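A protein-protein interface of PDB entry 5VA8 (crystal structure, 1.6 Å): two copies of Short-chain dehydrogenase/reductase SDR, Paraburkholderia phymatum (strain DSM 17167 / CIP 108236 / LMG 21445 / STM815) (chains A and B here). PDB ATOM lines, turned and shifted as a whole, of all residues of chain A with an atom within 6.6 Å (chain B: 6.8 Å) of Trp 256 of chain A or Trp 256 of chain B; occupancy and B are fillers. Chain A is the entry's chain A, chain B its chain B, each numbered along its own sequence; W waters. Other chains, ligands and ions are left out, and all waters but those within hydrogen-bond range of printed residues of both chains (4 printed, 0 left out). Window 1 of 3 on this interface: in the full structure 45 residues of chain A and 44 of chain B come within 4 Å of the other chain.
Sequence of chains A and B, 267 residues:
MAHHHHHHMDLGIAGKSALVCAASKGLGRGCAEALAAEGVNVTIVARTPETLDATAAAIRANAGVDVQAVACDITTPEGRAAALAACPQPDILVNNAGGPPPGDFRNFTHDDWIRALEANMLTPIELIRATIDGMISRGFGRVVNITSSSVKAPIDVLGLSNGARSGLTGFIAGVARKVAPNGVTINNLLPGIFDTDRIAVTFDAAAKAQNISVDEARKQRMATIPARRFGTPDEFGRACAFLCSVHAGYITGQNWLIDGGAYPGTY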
ATOM      1  N   THR A 147     -12.441 -16.419  24.281  1.00  0.00           N
ATOM      2  CA  THR A 147     -13.247 -17.069  25.309  1.00  0.00           C
ATOM      3  C   THR A 147     -12.582 -16.837  26.659  1.00  0.00           C
ATOM      4  O   THR A 147     -12.490 -15.681  27.091  1.00  0.00           O
ATOM      5  CB  THR A 147     -13.481 -18.557  24.999  1.00  0.00           C
ATOM      6  OG1 THR A 147     -12.244 -19.283  24.935  1.00  0.00           O
ATOM      7  CG2 THR A 147     -14.223 -18.699  23.654  1.00  0.00           C
ATOM      8  N   ASN A 187     -11.144 -21.056  15.398  1.00  0.00           N
ATOM      9  CA  ASN A 187     -10.365 -21.422  16.570  1.00  0.00           C
ATOM     10  C   ASN A 187     -10.748 -20.506  17.716  1.00  0.00           C
ATOM     11  O   ASN A 187     -11.317 -19.432  17.515  1.00  0.00           O
ATOM     12  CB  ASN A 187      -8.856 -21.315  16.307  1.00  0.00           C
ATOM     13  CG  ASN A 187      -8.388 -22.317  15.277  1.00  0.00           C
ATOM     14  OD1 ASN A 187      -8.349 -23.519  15.546  1.00  0.00           O
ATOM     15  ND2 ASN A 187      -8.014 -21.830  14.095  1.00  0.00           N
ATOM     16  N   ASN A 188     -10.424 -20.947  18.928  1.00  0.00           N
ATOM     17  CA  ASN A 188     -10.712 -20.177  20.129  1.00  0.00           C
ATOM     18  C   ASN A 188      -9.410 -19.784  20.809  1.00  0.00           C
ATOM     19  O   ASN A 188      -8.481 -20.590  20.902  1.00  0.00           O
ATOM     20  CB  ASN A 188     -11.595 -20.976  21.087  1.00  0.00           C
ATOM     21  CG  ASN A 188     -12.811 -21.564  20.389  1.00  0.00           C
ATOM     22  OD1 ASN A 188     -13.512 -20.864  19.662  1.00  0.00           O
ATOM     23  ND2 ASN A 188     -13.042 -22.861  20.576  1.00  0.00           N
ATOM     24  N   LEU A 189      -9.355 -18.538  21.278  1.00  0.00           N
ATOM     25  CA  LEU A 189      -8.239 -18.021  22.058  1.00  0.00           C
ATOM     26  C   LEU A 189      -8.709 -17.843  23.486  1.00  0.00           C
ATOM     27  O   LEU A 189      -9.644 -17.073  23.735  1.00  0.00           O
ATOM     28  CB  LEU A 189      -7.747 -16.686  21.500  1.00  0.00           C
ATOM     29  CG  LEU A 189      -6.666 -16.660  20.427  1.00  0.00           C
ATOM     30  CD1 LEU A 189      -6.261 -15.216  20.175  1.00  0.00           C
ATOM     31  CD2 LEU A 189      -5.452 -17.510  20.841  1.00  0.00           C
ATOM     32  N   LEU A 190      -8.063 -18.543  24.415  1.00  0.00           N
ATOM     33  CA  LEU A 190      -8.504 -18.622  25.805  1.00  0.00           C
ATOM     34  C   LEU A 190      -7.548 -17.829  26.680  1.00  0.00           C
ATOM     35  O   LEU A 190      -6.459 -18.330  27.021  1.00  0.00           O
ATOM     36  CB  LEU A 190      -8.549 -20.082  26.276  1.00  0.00           C
ATOM     37  CG  LEU A 190      -9.572 -21.079  25.715  1.00  0.00           C
ATOM     38  CD1 LEU A 190      -9.551 -21.180  24.192  1.00  0.00           C
ATOM     39  CD2 LEU A 190      -9.266 -22.452  26.298  1.00  0.00           C
ATOM     40  N   PRO A 191      -7.895 -16.608  27.092  1.00  0.00           N
ATOM     41  CA  PRO A 191      -6.988 -15.856  27.967  1.00  0.00           C
ATOM     42  C   PRO A 191      -7.016 -16.391  29.387  1.00  0.00           C
ATOM     43  O   PRO A 191      -8.079 -16.715  29.927  1.00  0.00           O
ATOM     44  CB  PRO A 191      -7.526 -14.415  27.921  1.00  0.00           C
ATOM     45  CG  PRO A 191      -8.743 -14.442  27.048  1.00  0.00           C
ATOM     46  CD  PRO A 191      -9.128 -15.870  26.780  1.00  0.00           C
ATOM     47  N   PHE A 236      -1.461 -11.074  23.122  1.00  0.00           N
ATOM     48  CA  PHE A 236      -2.709 -11.752  22.781  1.00  0.00           C
ATOM     49  C   PHE A 236      -3.089 -11.476  21.329  1.00  0.00           C
ATOM     50  O   PHE A 236      -3.422 -12.397  20.572  1.00  0.00           O
ATOM     51  CB  PHE A 236      -3.826 -11.293  23.723  1.00  0.00           C
ATOM     52  CG  PHE A 236      -5.093 -12.092  23.593  1.00  0.00           C
ATOM     53  CD1 PHE A 236      -5.232 -13.314  24.244  1.00  0.00           C
ATOM     54  CD2 PHE A 236      -6.140 -11.630  22.803  1.00  0.00           C
ATOM     55  CE1 PHE A 236      -6.405 -14.055  24.121  1.00  0.00           C
ATOM     56  CE2 PHE A 236      -7.311 -12.369  22.674  1.00  0.00           C
ATOM     57  CZ  PHE A 236      -7.442 -13.582  23.329  1.00  0.00           C
ATOM     58  N   ALA A 239      -0.963 -13.456  18.813  1.00  0.00           N
ATOM     59  CA  ALA A 239      -1.420 -14.832  18.626  1.00  0.00           C
ATOM     60  C   ALA A 239      -2.660 -14.878  17.744  1.00  0.00           C
ATOM     61  O   ALA A 239      -2.785 -15.748  16.876  1.00  0.00           O
ATOM     62  CB  ALA A 239      -1.704 -15.492  19.974  1.00  0.00           C
ATOM     63  N   CYS A 240      -3.583 -13.937  17.945  1.00  0.00           N
ATOM     64  CA  CYS A 240      -4.743 -13.840  17.070  1.00  0.00           C
ATOM     65  C   CYS A 240      -4.318 -13.639  15.617  1.00  0.00           C
ATOM     66  O   CYS A 240      -4.831 -14.301  14.708  1.00  0.00           O
ATOM     67  CB  CYS A 240      -5.635 -12.691  17.534  1.00  0.00           C
ATOM     68  SG  CYS A 240      -7.145 -12.485  16.554  1.00  0.00           S
ATOM     69  N   PHE A 242      -1.539 -14.485  14.172  1.00  0.00           N
ATOM     70  CA  PHE A 242      -0.987 -15.711  13.602  1.00  0.00           C
ATOM     71  C   PHE A 242      -2.097 -16.675  13.182  1.00  0.00           C
ATOM     72  O   PHE A 242      -2.044 -17.254  12.087  1.00  0.00           O
ATOM     73  CB  PHE A 242      -0.030 -16.399  14.572  1.00  0.00           C
ATOM     74  CG  PHE A 242       0.623 -17.600  13.961  1.00  0.00           C
ATOM     75  CD1 PHE A 242       1.702 -17.440  13.114  1.00  0.00           C
ATOM     76  CD2 PHE A 242       0.089 -18.865  14.139  1.00  0.00           C
ATOM     77  CE1 PHE A 242       2.300 -18.542  12.499  1.00  0.00           C
ATOM     78  CE2 PHE A 242       0.677 -19.969  13.520  1.00  0.00           C
ATOM     79  CZ  PHE A 242       1.775 -19.800  12.705  1.00  0.00           C
ATOM     80  N   LEU A 243      -3.112 -16.860  14.034  1.00  0.00           N
ATOM     81  CA  LEU A 243      -4.227 -17.729  13.659  1.00  0.00           C
ATOM     82  C   LEU A 243      -4.921 -17.226  12.406  1.00  0.00           C
ATOM     83  O   LEU A 243      -5.429 -18.026  11.608  1.00  0.00           O
ATOM     84  CB  LEU A 243      -5.251 -17.829  14.791  1.00  0.00           C
ATOM     85  CG  LEU A 243      -4.883 -18.721  15.975  1.00  0.00           C
ATOM     86  CD1 LEU A 243      -5.914 -18.538  17.083  1.00  0.00           C
ATOM     87  CD2 LEU A 243      -4.785 -20.186  15.556  1.00  0.00           C
ATOM     88  N   ALA A 248      -1.585 -20.485   9.180  1.00  0.00           N
ATOM     89  CA  ALA A 248      -2.358 -21.229  10.162  1.00  0.00           C
ATOM     90  C   ALA A 248      -3.538 -21.951   9.523  1.00  0.00           C
ATOM     91  O   ALA A 248      -4.498 -22.303  10.215  1.00  0.00           O
ATOM     92  CB  ALA A 248      -2.838 -20.296  11.275  1.00  0.00           C
ATOM     93  N   ILE A 251      -4.739 -25.300  11.124  1.00  0.00           N
ATOM     94  CA  ILE A 251      -5.142 -25.245  12.527  1.00  0.00           C
ATOM     95  C   ILE A 251      -6.621 -24.890  12.539  1.00  0.00           C
ATOM     96  O   ILE A 251      -6.998 -23.773  12.152  1.00  0.00           O
ATOM     97  CB  ILE A 251      -4.323 -24.208  13.308  1.00  0.00           C
ATOM     98  CG1 ILE A 251      -2.821 -24.507  13.199  1.00  0.00           C
ATOM     99  CG2 ILE A 251      -4.771 -24.160  14.768  1.00  0.00           C
ATOM    100  CD1 ILE A 251      -1.916 -23.375  13.682  1.00  0.00           C
ATOM    101  N   GLN A 254      -9.274 -25.612  17.321  1.00  0.00           N
ATOM    102  CA  GLN A 254      -8.317 -25.671  18.419  1.00  0.00           C
ATOM    103  C   GLN A 254      -8.604 -24.601  19.460  1.00  0.00           C
ATOM    104  O   GLN A 254      -9.063 -23.495  19.144  1.00  0.00           O
ATOM    105  CB  GLN A 254      -6.886 -25.519  17.904  1.00  0.00           C
ATOM    106  CG  GLN A 254      -6.479 -26.664  16.953  1.00  0.00           C
ATOM    107  CD  GLN A 254      -6.854 -28.044  17.497  1.00  0.00           C
ATOM    108  OE1 GLN A 254      -6.394 -28.445  18.577  1.00  0.00           O
ATOM    109  NE2 GLN A 254      -7.703 -28.763  16.766  1.00  0.00           N
ATOM    110  N   ASN A 255      -8.327 -24.957  20.712  1.00  0.00           N
ATOM    111  CA  ASN A 255      -8.466 -24.066  21.857  1.00  0.00           C
ATOM    112  C   ASN A 255      -7.060 -23.714  22.313  1.00  0.00           C
ATOM    113  O   ASN A 255      -6.378 -24.535  22.928  1.00  0.00           O
ATOM    114  CB  ASN A 255      -9.279 -24.747  22.952  1.00  0.00           C
ATOM    115  CG  ASN A 255     -10.727 -24.871  22.563  1.00  0.00           C
ATOM    116  OD1 ASN A 255     -11.487 -23.913  22.681  1.00  0.00           O
ATOM    117  ND2 ASN A 255     -11.112 -26.031  22.035  1.00  0.00           N
ATOM    118  N   TRP A 256      -6.624 -22.495  21.998  1.00  0.00           N
ATOM    119  CA  TRP A 256      -5.277 -22.040  22.344  1.00  0.00           C
ATOM    120  C   TRP A 256      -5.346 -21.309  23.676  1.00  0.00           C
ATOM    121  O   TRP A 256      -5.874 -20.199  23.750  1.00  0.00           O
ATOM    122  CB  TRP A 256      -4.710 -21.119  21.267  1.00  0.00           C
ATOM    123  CG  TRP A 256      -4.037 -21.822  20.113  1.00  0.00           C
ATOM    124  CD1 TRP A 256      -4.079 -23.141  19.815  1.00  0.00           C
ATOM    125  CD2 TRP A 256      -3.203 -21.206  19.125  1.00  0.00           C
ATOM    126  NE1 TRP A 256      -3.315 -23.400  18.683  1.00  0.00           N
ATOM    127  CE2 TRP A 256      -2.765 -22.224  18.252  1.00  0.00           C
ATOM    128  CE3 TRP A 256      -2.774 -19.896  18.907  1.00  0.00           C
ATOM    129  CZ2 TRP A 256      -1.920 -21.967  17.170  1.00  0.00           C
ATOM    130  CZ3 TRP A 256      -1.935 -19.644  17.830  1.00  0.00           C
ATOM    131  CH2 TRP A 256      -1.522 -20.674  16.980  1.00  0.00           C
ATOM    132  N   LEU A 257      -4.796 -21.921  24.718  1.00  0.00           N
ATOM    133  CA  LEU A 257      -4.780 -21.320  26.044  1.00  0.00           C
ATOM    134  C   LEU A 257      -3.514 -20.480  26.186  1.00  0.00           C
ATOM    135  O   LEU A 257      -2.400 -20.985  25.986  1.00  0.00           O
ATOM    136  CB  LEU A 257      -4.843 -22.422  27.098  1.00  0.00           C
ATOM    137  CG  LEU A 257      -4.789 -22.045  28.568  1.00  0.00           C
ATOM    138  CD1 LEU A 257      -6.001 -21.215  28.948  1.00  0.00           C
ATOM    139  CD2 LEU A 257      -4.709 -23.323  29.395  1.00  0.00           C
ATOM    140  N   ILE A 258      -3.684 -19.204  26.511  1.00  0.00           N
ATOM    141  CA  ILE A 258      -2.572 -18.264  26.642  1.00  0.00           C
ATOM    142  C   ILE A 258      -2.643 -17.751  28.075  1.00  0.00           C
ATOM    143  O   ILE A 258      -3.350 -16.775  28.366  1.00  0.00           O
ATOM    144  CB  ILE A 258      -2.645 -17.121  25.625  1.00  0.00           C
ATOM    145  CG1 ILE A 258      -2.800 -17.678  24.209  1.00  0.00           C
ATOM    146  CG2 ILE A 258      -1.392 -16.258  25.682  1.00  0.00           C
ATOM    147  CD1 ILE A 258      -2.734 -16.611  23.153  1.00  0.00           C
ATOM    148  N   THR B 147       5.947 -33.776  18.482  1.00  0.00           N
ATOM    149  CA  THR B 147       5.434 -35.071  18.915  1.00  0.00           C
ATOM    150  C   THR B 147       4.517 -35.636  17.836  1.00  0.00           C
ATOM    151  O   THR B 147       5.000 -35.962  16.751  1.00  0.00           O
ATOM    152  CB  THR B 147       4.736 -34.978  20.277  1.00  0.00           C
ATOM    153  OG1 THR B 147       3.637 -34.067  20.206  1.00  0.00           O
ATOM    154  CG2 THR B 147       5.719 -34.481  21.344  1.00  0.00           C
ATOM    155  N   ASN B 187       6.779 -26.093  24.942  1.00  0.00           N
ATOM    156  CA  ASN B 187       5.512 -26.423  24.308  1.00  0.00           C
ATOM    157  C   ASN B 187       5.738 -27.563  23.334  1.00  0.00           C
ATOM    158  O   ASN B 187       6.865 -27.834  22.914  1.00  0.00           O
ATOM    159  CB  ASN B 187       4.910 -25.221  23.564  1.00  0.00           C
ATOM    160  CG  ASN B 187       4.538 -24.079  24.502  1.00  0.00           C
ATOM    161  OD1 ASN B 187       3.553 -24.161  25.252  1.00  0.00           O
ATOM    162  ND2 ASN B 187       5.309 -23.002  24.447  1.00  0.00           N
ATOM    163  N   ASN B 188       4.642 -28.223  22.975  1.00  0.00           N
ATOM    164  CA  ASN B 188       4.689 -29.359  22.063  1.00  0.00           C
ATOM    165  C   ASN B 188       3.880 -29.036  20.820  1.00  0.00           C
ATOM    166  O   ASN B 188       2.778 -28.486  20.909  1.00  0.00           O
ATOM    167  CB  ASN B 188       4.129 -30.618  22.708  1.00  0.00           C
ATOM    168  CG  ASN B 188       4.739 -30.882  24.050  1.00  0.00           C
ATOM    169  OD1 ASN B 188       5.957 -30.826  24.203  1.00  0.00           O
ATOM    170  ND2 ASN B 188       3.901 -31.146  25.043  1.00  0.00           N
ATOM    171  N   LEU B 189       4.425 -29.417  19.671  1.00  0.00           N
ATOM    172  CA  LEU B 189       3.752 -29.261  18.385  1.00  0.00           C
ATOM    173  C   LEU B 189       3.388 -30.652  17.895  1.00  0.00           C
ATOM    174  O   LEU B 189       4.271 -31.500  17.725  1.00  0.00           O
ATOM    175  CB  LEU B 189       4.646 -28.555  17.368  1.00  0.00           C
ATOM    176  CG  LEU B 189       4.683 -27.038  17.219  1.00  0.00           C
ATOM    177  CD1 LEU B 189       5.535 -26.674  16.009  1.00  0.00           C
ATOM    178  CD2 LEU B 189       3.275 -26.452  17.085  1.00  0.00           C
ATOM    179  N   LEU B 190       2.094 -30.880  17.680  1.00  0.00           N
ATOM    180  CA  LEU B 190       1.554 -32.207  17.404  1.00  0.00           C
ATOM    181  C   LEU B 190       1.108 -32.253  15.952  1.00  0.00           C
ATOM    182  O   LEU B 190       0.025 -31.748  15.624  1.00  0.00           O
ATOM    183  CB  LEU B 190       0.366 -32.507  18.326  1.00  0.00           C
ATOM    184  CG  LEU B 190       0.582 -32.734  19.828  1.00  0.00           C
ATOM    185  CD1 LEU B 190       1.290 -31.577  20.528  1.00  0.00           C
ATOM    186  CD2 LEU B 190      -0.784 -32.962  20.476  1.00  0.00           C
ATOM    187  N   PRO B 191       1.895 -32.820  15.043  1.00  0.00           N
ATOM    188  CA  PRO B 191       1.450 -32.877  13.646  1.00  0.00           C
ATOM    189  C   PRO B 191       0.392 -33.945  13.435  1.00  0.00           C
ATOM    190  O   PRO B 191       0.474 -35.047  13.983  1.00  0.00           O
ATOM    191  CB  PRO B 191       2.731 -33.206  12.862  1.00  0.00           C
ATOM    192  CG  PRO B 191       3.734 -33.665  13.874  1.00  0.00           C
ATOM    193  CD  PRO B 191       3.251 -33.359  15.250  1.00  0.00           C
ATOM    194  N   PHE B 236       4.198 -25.827   9.345  1.00  0.00           N
ATOM    195  CA  PHE B 236       4.624 -26.386  10.621  1.00  0.00           C
ATOM    196  C   PHE B 236       5.773 -25.574  11.206  1.00  0.00           C
ATOM    197  O   PHE B 236       5.752 -25.199  12.385  1.00  0.00           O
ATOM    198  CB  PHE B 236       5.032 -27.845  10.434  1.00  0.00           C
ATOM    199  CG  PHE B 236       5.253 -28.573  11.729  1.00  0.00           C
ATOM    200  CD1 PHE B 236       4.173 -29.114  12.418  1.00  0.00           C
ATOM    201  CD2 PHE B 236       6.525 -28.685  12.271  1.00  0.00           C
ATOM    202  CE1 PHE B 236       4.363 -29.783  13.622  1.00  0.00           C
ATOM    203  CE2 PHE B 236       6.737 -29.352  13.487  1.00  0.00           C
ATOM    204  CZ  PHE B 236       5.653 -29.901  14.167  1.00  0.00           C
ATOM    205  N   ALA B 239       4.600 -22.176  12.663  1.00  0.00           N
ATOM    206  CA  ALA B 239       4.039 -22.298  14.005  1.00  0.00           C
ATOM    207  C   ALA B 239       5.142 -22.476  15.038  1.00  0.00           C
ATOM    208  O   ALA B 239       5.102 -21.873  16.115  1.00  0.00           O
ATOM    209  CB  ALA B 239       3.058 -23.466  14.065  1.00  0.00           C
ATOM    210  N   CYS B 240       6.149 -23.282  14.713  1.00  0.00           N
ATOM    211  CA  CYS B 240       7.305 -23.414  15.592  1.00  0.00           C
ATOM    212  C   CYS B 240       7.965 -22.060  15.841  1.00  0.00           C
ATOM    213  O   CYS B 240       8.278 -21.708  16.986  1.00  0.00           O
ATOM    214  CB  CYS B 240       8.310 -24.391  14.982  1.00  0.00           C
ATOM    215  SG  CYS B 240       9.751 -24.698  16.031  1.00  0.00           S
ATOM    216  N   PHE B 242       6.694 -19.060  15.645  1.00  0.00           N
ATOM    217  CA  PHE B 242       5.882 -18.204  16.505  1.00  0.00           C
ATOM    218  C   PHE B 242       6.046 -18.592  17.970  1.00  0.00           C
ATOM    219  O   PHE B 242       6.175 -17.720  18.836  1.00  0.00           O
ATOM    220  CB  PHE B 242       4.403 -18.252  16.112  1.00  0.00           C
ATOM    221  CG  PHE B 242       3.559 -17.316  16.937  1.00  0.00           C
ATOM    222  CD1 PHE B 242       3.462 -15.976  16.604  1.00  0.00           C
ATOM    223  CD2 PHE B 242       2.946 -17.760  18.102  1.00  0.00           C
ATOM    224  CE1 PHE B 242       2.717 -15.100  17.386  1.00  0.00           C
ATOM    225  CE2 PHE B 242       2.212 -16.894  18.889  1.00  0.00           C
ATOM    226  CZ  PHE B 242       2.092 -15.563  18.534  1.00  0.00           C
ATOM    227  N   LEU B 243       6.027 -19.894  18.273  1.00  0.00           N
ATOM    228  CA  LEU B 243       6.233 -20.315  19.661  1.00  0.00           C
ATOM    229  C   LEU B 243       7.591 -19.875  20.189  1.00  0.00           C
ATOM    230  O   LEU B 243       7.726 -19.551  21.374  1.00  0.00           O
ATOM    231  CB  LEU B 243       6.097 -21.834  19.782  1.00  0.00           C
ATOM    232  CG  LEU B 243       4.672 -22.386  19.744  1.00  0.00           C
ATOM    233  CD1 LEU B 243       4.714 -23.913  19.601  1.00  0.00           C
ATOM    234  CD2 LEU B 243       3.895 -21.959  20.994  1.00  0.00           C
ATOM    235  N   ALA B 248       5.295 -15.073  22.247  1.00  0.00           N
ATOM    236  CA  ALA B 248       4.680 -16.282  22.778  1.00  0.00           C
ATOM    237  C   ALA B 248       5.172 -16.573  24.189  1.00  0.00           C
ATOM    238  O   ALA B 248       5.114 -17.717  24.649  1.00  0.00           O
ATOM    239  CB  ALA B 248       4.950 -17.469  21.851  1.00  0.00           C
ATOM    240  N   ILE B 251       2.771 -18.388  26.628  1.00  0.00           N
ATOM    241  CA  ILE B 251       2.292 -19.690  26.190  1.00  0.00           C
ATOM    242  C   ILE B 251       3.303 -20.715  26.673  1.00  0.00           C
ATOM    243  O   ILE B 251       4.451 -20.726  26.210  1.00  0.00           O
ATOM    244  CB  ILE B 251       2.136 -19.752  24.665  1.00  0.00           C
ATOM    245  CG1 ILE B 251       1.224 -18.622  24.167  1.00  0.00           C
ATOM    246  CG2 ILE B 251       1.640 -21.147  24.238  1.00  0.00           C
ATOM    247  CD1 ILE B 251       1.170 -18.541  22.650  1.00  0.00           C
ATOM    248  N   GLN B 254       1.781 -26.025  26.540  1.00  0.00           N
ATOM    249  CA  GLN B 254       0.652 -26.229  25.647  1.00  0.00           C
ATOM    250  C   GLN B 254       0.973 -27.258  24.576  1.00  0.00           C
ATOM    251  O   GLN B 254       2.114 -27.379  24.115  1.00  0.00           O
ATOM    252  CB  GLN B 254       0.231 -24.915  24.999  1.00  0.00           C
ATOM    253  CG  GLN B 254      -0.200 -23.891  26.027  1.00  0.00           C
ATOM    254  CD  GLN B 254      -1.202 -24.461  27.014  1.00  0.00           C
ATOM    255  OE1 GLN B 254      -2.280 -24.891  26.620  1.00  0.00           O
ATOM    256  NE2 GLN B 254      -0.852 -24.470  28.302  1.00  0.00           N
ATOM    257  N   ASN B 255      -0.061 -28.004  24.192  1.00  0.00           N
ATOM    258  CA  ASN B 255       0.001 -28.998  23.125  1.00  0.00           C
ATOM    259  C   ASN B 255      -0.773 -28.446  21.945  1.00  0.00           C
ATOM    260  O   ASN B 255      -2.009 -28.425  21.963  1.00  0.00           O
ATOM    261  CB  ASN B 255      -0.578 -30.321  23.596  1.00  0.00           C
ATOM    262  CG  ASN B 255       0.321 -31.001  24.584  1.00  0.00           C
ATOM    263  OD1 ASN B 255       1.301 -31.625  24.200  1.00  0.00           O
ATOM    264  ND2 ASN B 255       0.028 -30.835  25.878  1.00  0.00           N
ATOM    265  N   TRP B 256      -0.049 -27.975  20.934  1.00  0.00           N
ATOM    266  CA  TRP B 256      -0.653 -27.355  19.759  1.00  0.00           C
ATOM    267  C   TRP B 256      -0.805 -28.413  18.675  1.00  0.00           C
ATOM    268  O   TRP B 256       0.187 -28.838  18.072  1.00  0.00           O
ATOM    269  CB  TRP B 256       0.185 -26.192  19.250  1.00  0.00           C
ATOM    270  CG  TRP B 256      -0.088 -24.906  19.966  1.00  0.00           C
ATOM    271  CD1 TRP B 256      -0.830 -24.733  21.092  1.00  0.00           C
ATOM    272  CD2 TRP B 256       0.370 -23.616  19.574  1.00  0.00           C
ATOM    273  NE1 TRP B 256      -0.863 -23.395  21.437  1.00  0.00           N
ATOM    274  CE2 TRP B 256      -0.134 -22.691  20.518  1.00  0.00           C
ATOM    275  CE3 TRP B 256       1.163 -23.151  18.524  1.00  0.00           C
ATOM    276  CZ2 TRP B 256       0.133 -21.329  20.435  1.00  0.00           C
ATOM    277  CZ3 TRP B 256       1.423 -21.794  18.444  1.00  0.00           C
ATOM    278  CH2 TRP B 256       0.915 -20.907  19.395  1.00  0.00           C
ATOM    279  N   LEU B 257      -2.045 -28.804  18.414  1.00  0.00           N
ATOM    280  CA  LEU B 257      -2.358 -29.795  17.393  1.00  0.00           C
ATOM    281  C   LEU B 257      -2.562 -29.080  16.059  1.00  0.00           C
ATOM    282  O   LEU B 257      -3.400 -28.179  15.957  1.00  0.00           O
ATOM    283  CB  LEU B 257      -3.607 -30.573  17.805  1.00  0.00           C
ATOM    284  CG  LEU B 257      -4.166 -31.644  16.872  1.00  0.00           C
ATOM    285  CD1 LEU B 257      -3.150 -32.769  16.705  1.00  0.00           C
ATOM    286  CD2 LEU B 257      -5.502 -32.161  17.420  1.00  0.00           C
ATOM    287  N   ILE B 258      -1.803 -29.477  15.051  1.00  0.00           N
ATOM    288  CA  ILE B 258      -1.872 -28.853  13.731  1.00  0.00           C
ATOM    289  C   ILE B 258      -2.236 -29.985  12.779  1.00  0.00           C
ATOM    290  O   ILE B 258      -1.366 -30.731  12.322  1.00  0.00           O
ATOM    291  CB  ILE B 258      -0.557 -28.177  13.339  1.00  0.00           C
ATOM    292  CG1 ILE B 258      -0.129 -27.182  14.420  1.00  0.00           C
ATOM    293  CG2 ILE B 258      -0.667 -27.475  11.980  1.00  0.00           C
ATOM    294  CD1 ILE B 258       1.156 -26.469  14.091  1.00  0.00           C
HETATM  295  O   HOH W   1      -3.203 -24.302  24.188  1.00  0.00           O
HETATM  296  O   HOH W   2      -4.197 -27.223  19.613  1.00  0.00           O
HETATM  297  O   HOH W   3      -3.100 -25.889  17.730  1.00  0.00           O
HETATM  298  O   HOH W   4      -1.948 -22.213  23.412  1.00  0.00           O
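Water W4 bridges the indole nitrogen of Trp 256 of chain B and the backbone carbonyl oxygen of Leu 257 of chain A.
Water W1 lies within hydrogen-bond range of OE1 of Gln 254 of chain B, N of Leu 257 of chain A and O of Asn 255 of chain A.
Water W3 lies within hydrogen-bond range of the indole nitrogen (NE1) of Trp 256 of chain A (2.7 Å) and the backbone carbonyl oxygen (O) of Leu 257 of chain B (2.9 Å).
Water W2 lies within hydrogen-bond range of OE1 of Gln 254 of chain A, N of Leu 257 of chain B and O of Asn 255 of chain B.
Among the printed residues, merely in contact across the chains: Trp 256 of chain A with Trp 256 of chain B, Gln 254 of chain A with Leu 257 of chain B, Ala 239 of chain A with Phe 242 of chain B, Leu 257 of chain A with Gln 254 of chain B, Phe 242 of chain A with Ala 239 of chain B, Ile 258 of chain A with Ile 251 of chain B and Ile 251 of chain A with Ile 258 of chain B.
O of Leu 190 of chain B lies within hydrogen-bond range of N of Ile 258 of chain B (3.0 Å).
The backbone carbonyl oxygen (O) of Ile 251 of chain A is in hydrogen-bond range of the side-chain amide nitrogen (ND2) of Asn 187 of chain A, at 2.9 Å.
OD1 of Asn 187 of chain B sits at hydrogen-bond distance from N of Gln 254 of chain B (2.9 Å).
The backbone carbonyl oxygen (O) of Trp 256 of chain A is in hydrogen-bond range of the backbone NH (N) of Leu 190 of chain A (2.8 Å).
N of Leu 190 of chain B is in hydrogen-bond range of O of Trp 256 of chain B (2.8 Å).
Of the 18 printed residues of chain A, 7 touch a printed residue of chain B.
Printed residues of chain A that touch a printed residue of chain B: Ala 239, Phe 242, Ile 251, Gln 254, Trp 256, Leu 257 and Ile 258.
Hydrophobic or aromatic side chains of chain A that line the printed part of chain B: Phe 242, Ile 251, Trp 256, Leu 257 and Ile 258.
Along chain A the printed residues that touch a printed residue of chain B span positions 239 to 258.
Among the printed residues, 7 pairs touch across the chains.
Among the printed residues, no Asp or Glu carboxylate lies within 4 Å of a Lys or Arg side-chain nitrogen of the other chain.
Ala 248 of chain A touches none of the printed residues of chain B.
Of the printed residues of chain B, Gln 254 of chain A touches Leu 257 (3.6 Å).
Trp 256 of chain A touches just one residue of chain B: Trp 256.
Printed residues of chain B within 4 Å of Ile 258 of chain A: Ile 251 (3.8 Å).
Asn 188 of chain B touches none of the printed residues of chain A.
Of chain A, only Trp 256 (3.4 Å) comes within 4 Å of Trp 256 of chain B.
Printed residues of chain A within 4 Å of Leu 257 of chain B: Gln 254 (3.6 Å).
Ala 239 of chain A touches Phe 242 of chain B, and with the chains exchanged Phe 242 of chain A touches Ala 239 of chain B.
Gln 254 of chain A touches Leu 257 of chain B, and with the chains exchanged Leu 257 of chain A touches Gln 254 of chain B.
Trp 256 of chain A touches its own counterpart, Trp 256 of chain B.
Positions printed for both chains: 147, 187, 188, 189, 190, 191, 236, 239, 240, 242, 243, 248, 251, 254, 255, 256, 257 and 258.
Of the 7 pairs that touch across the chains among the printed residues, 7 have their exchanged pair printed and touching as well.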
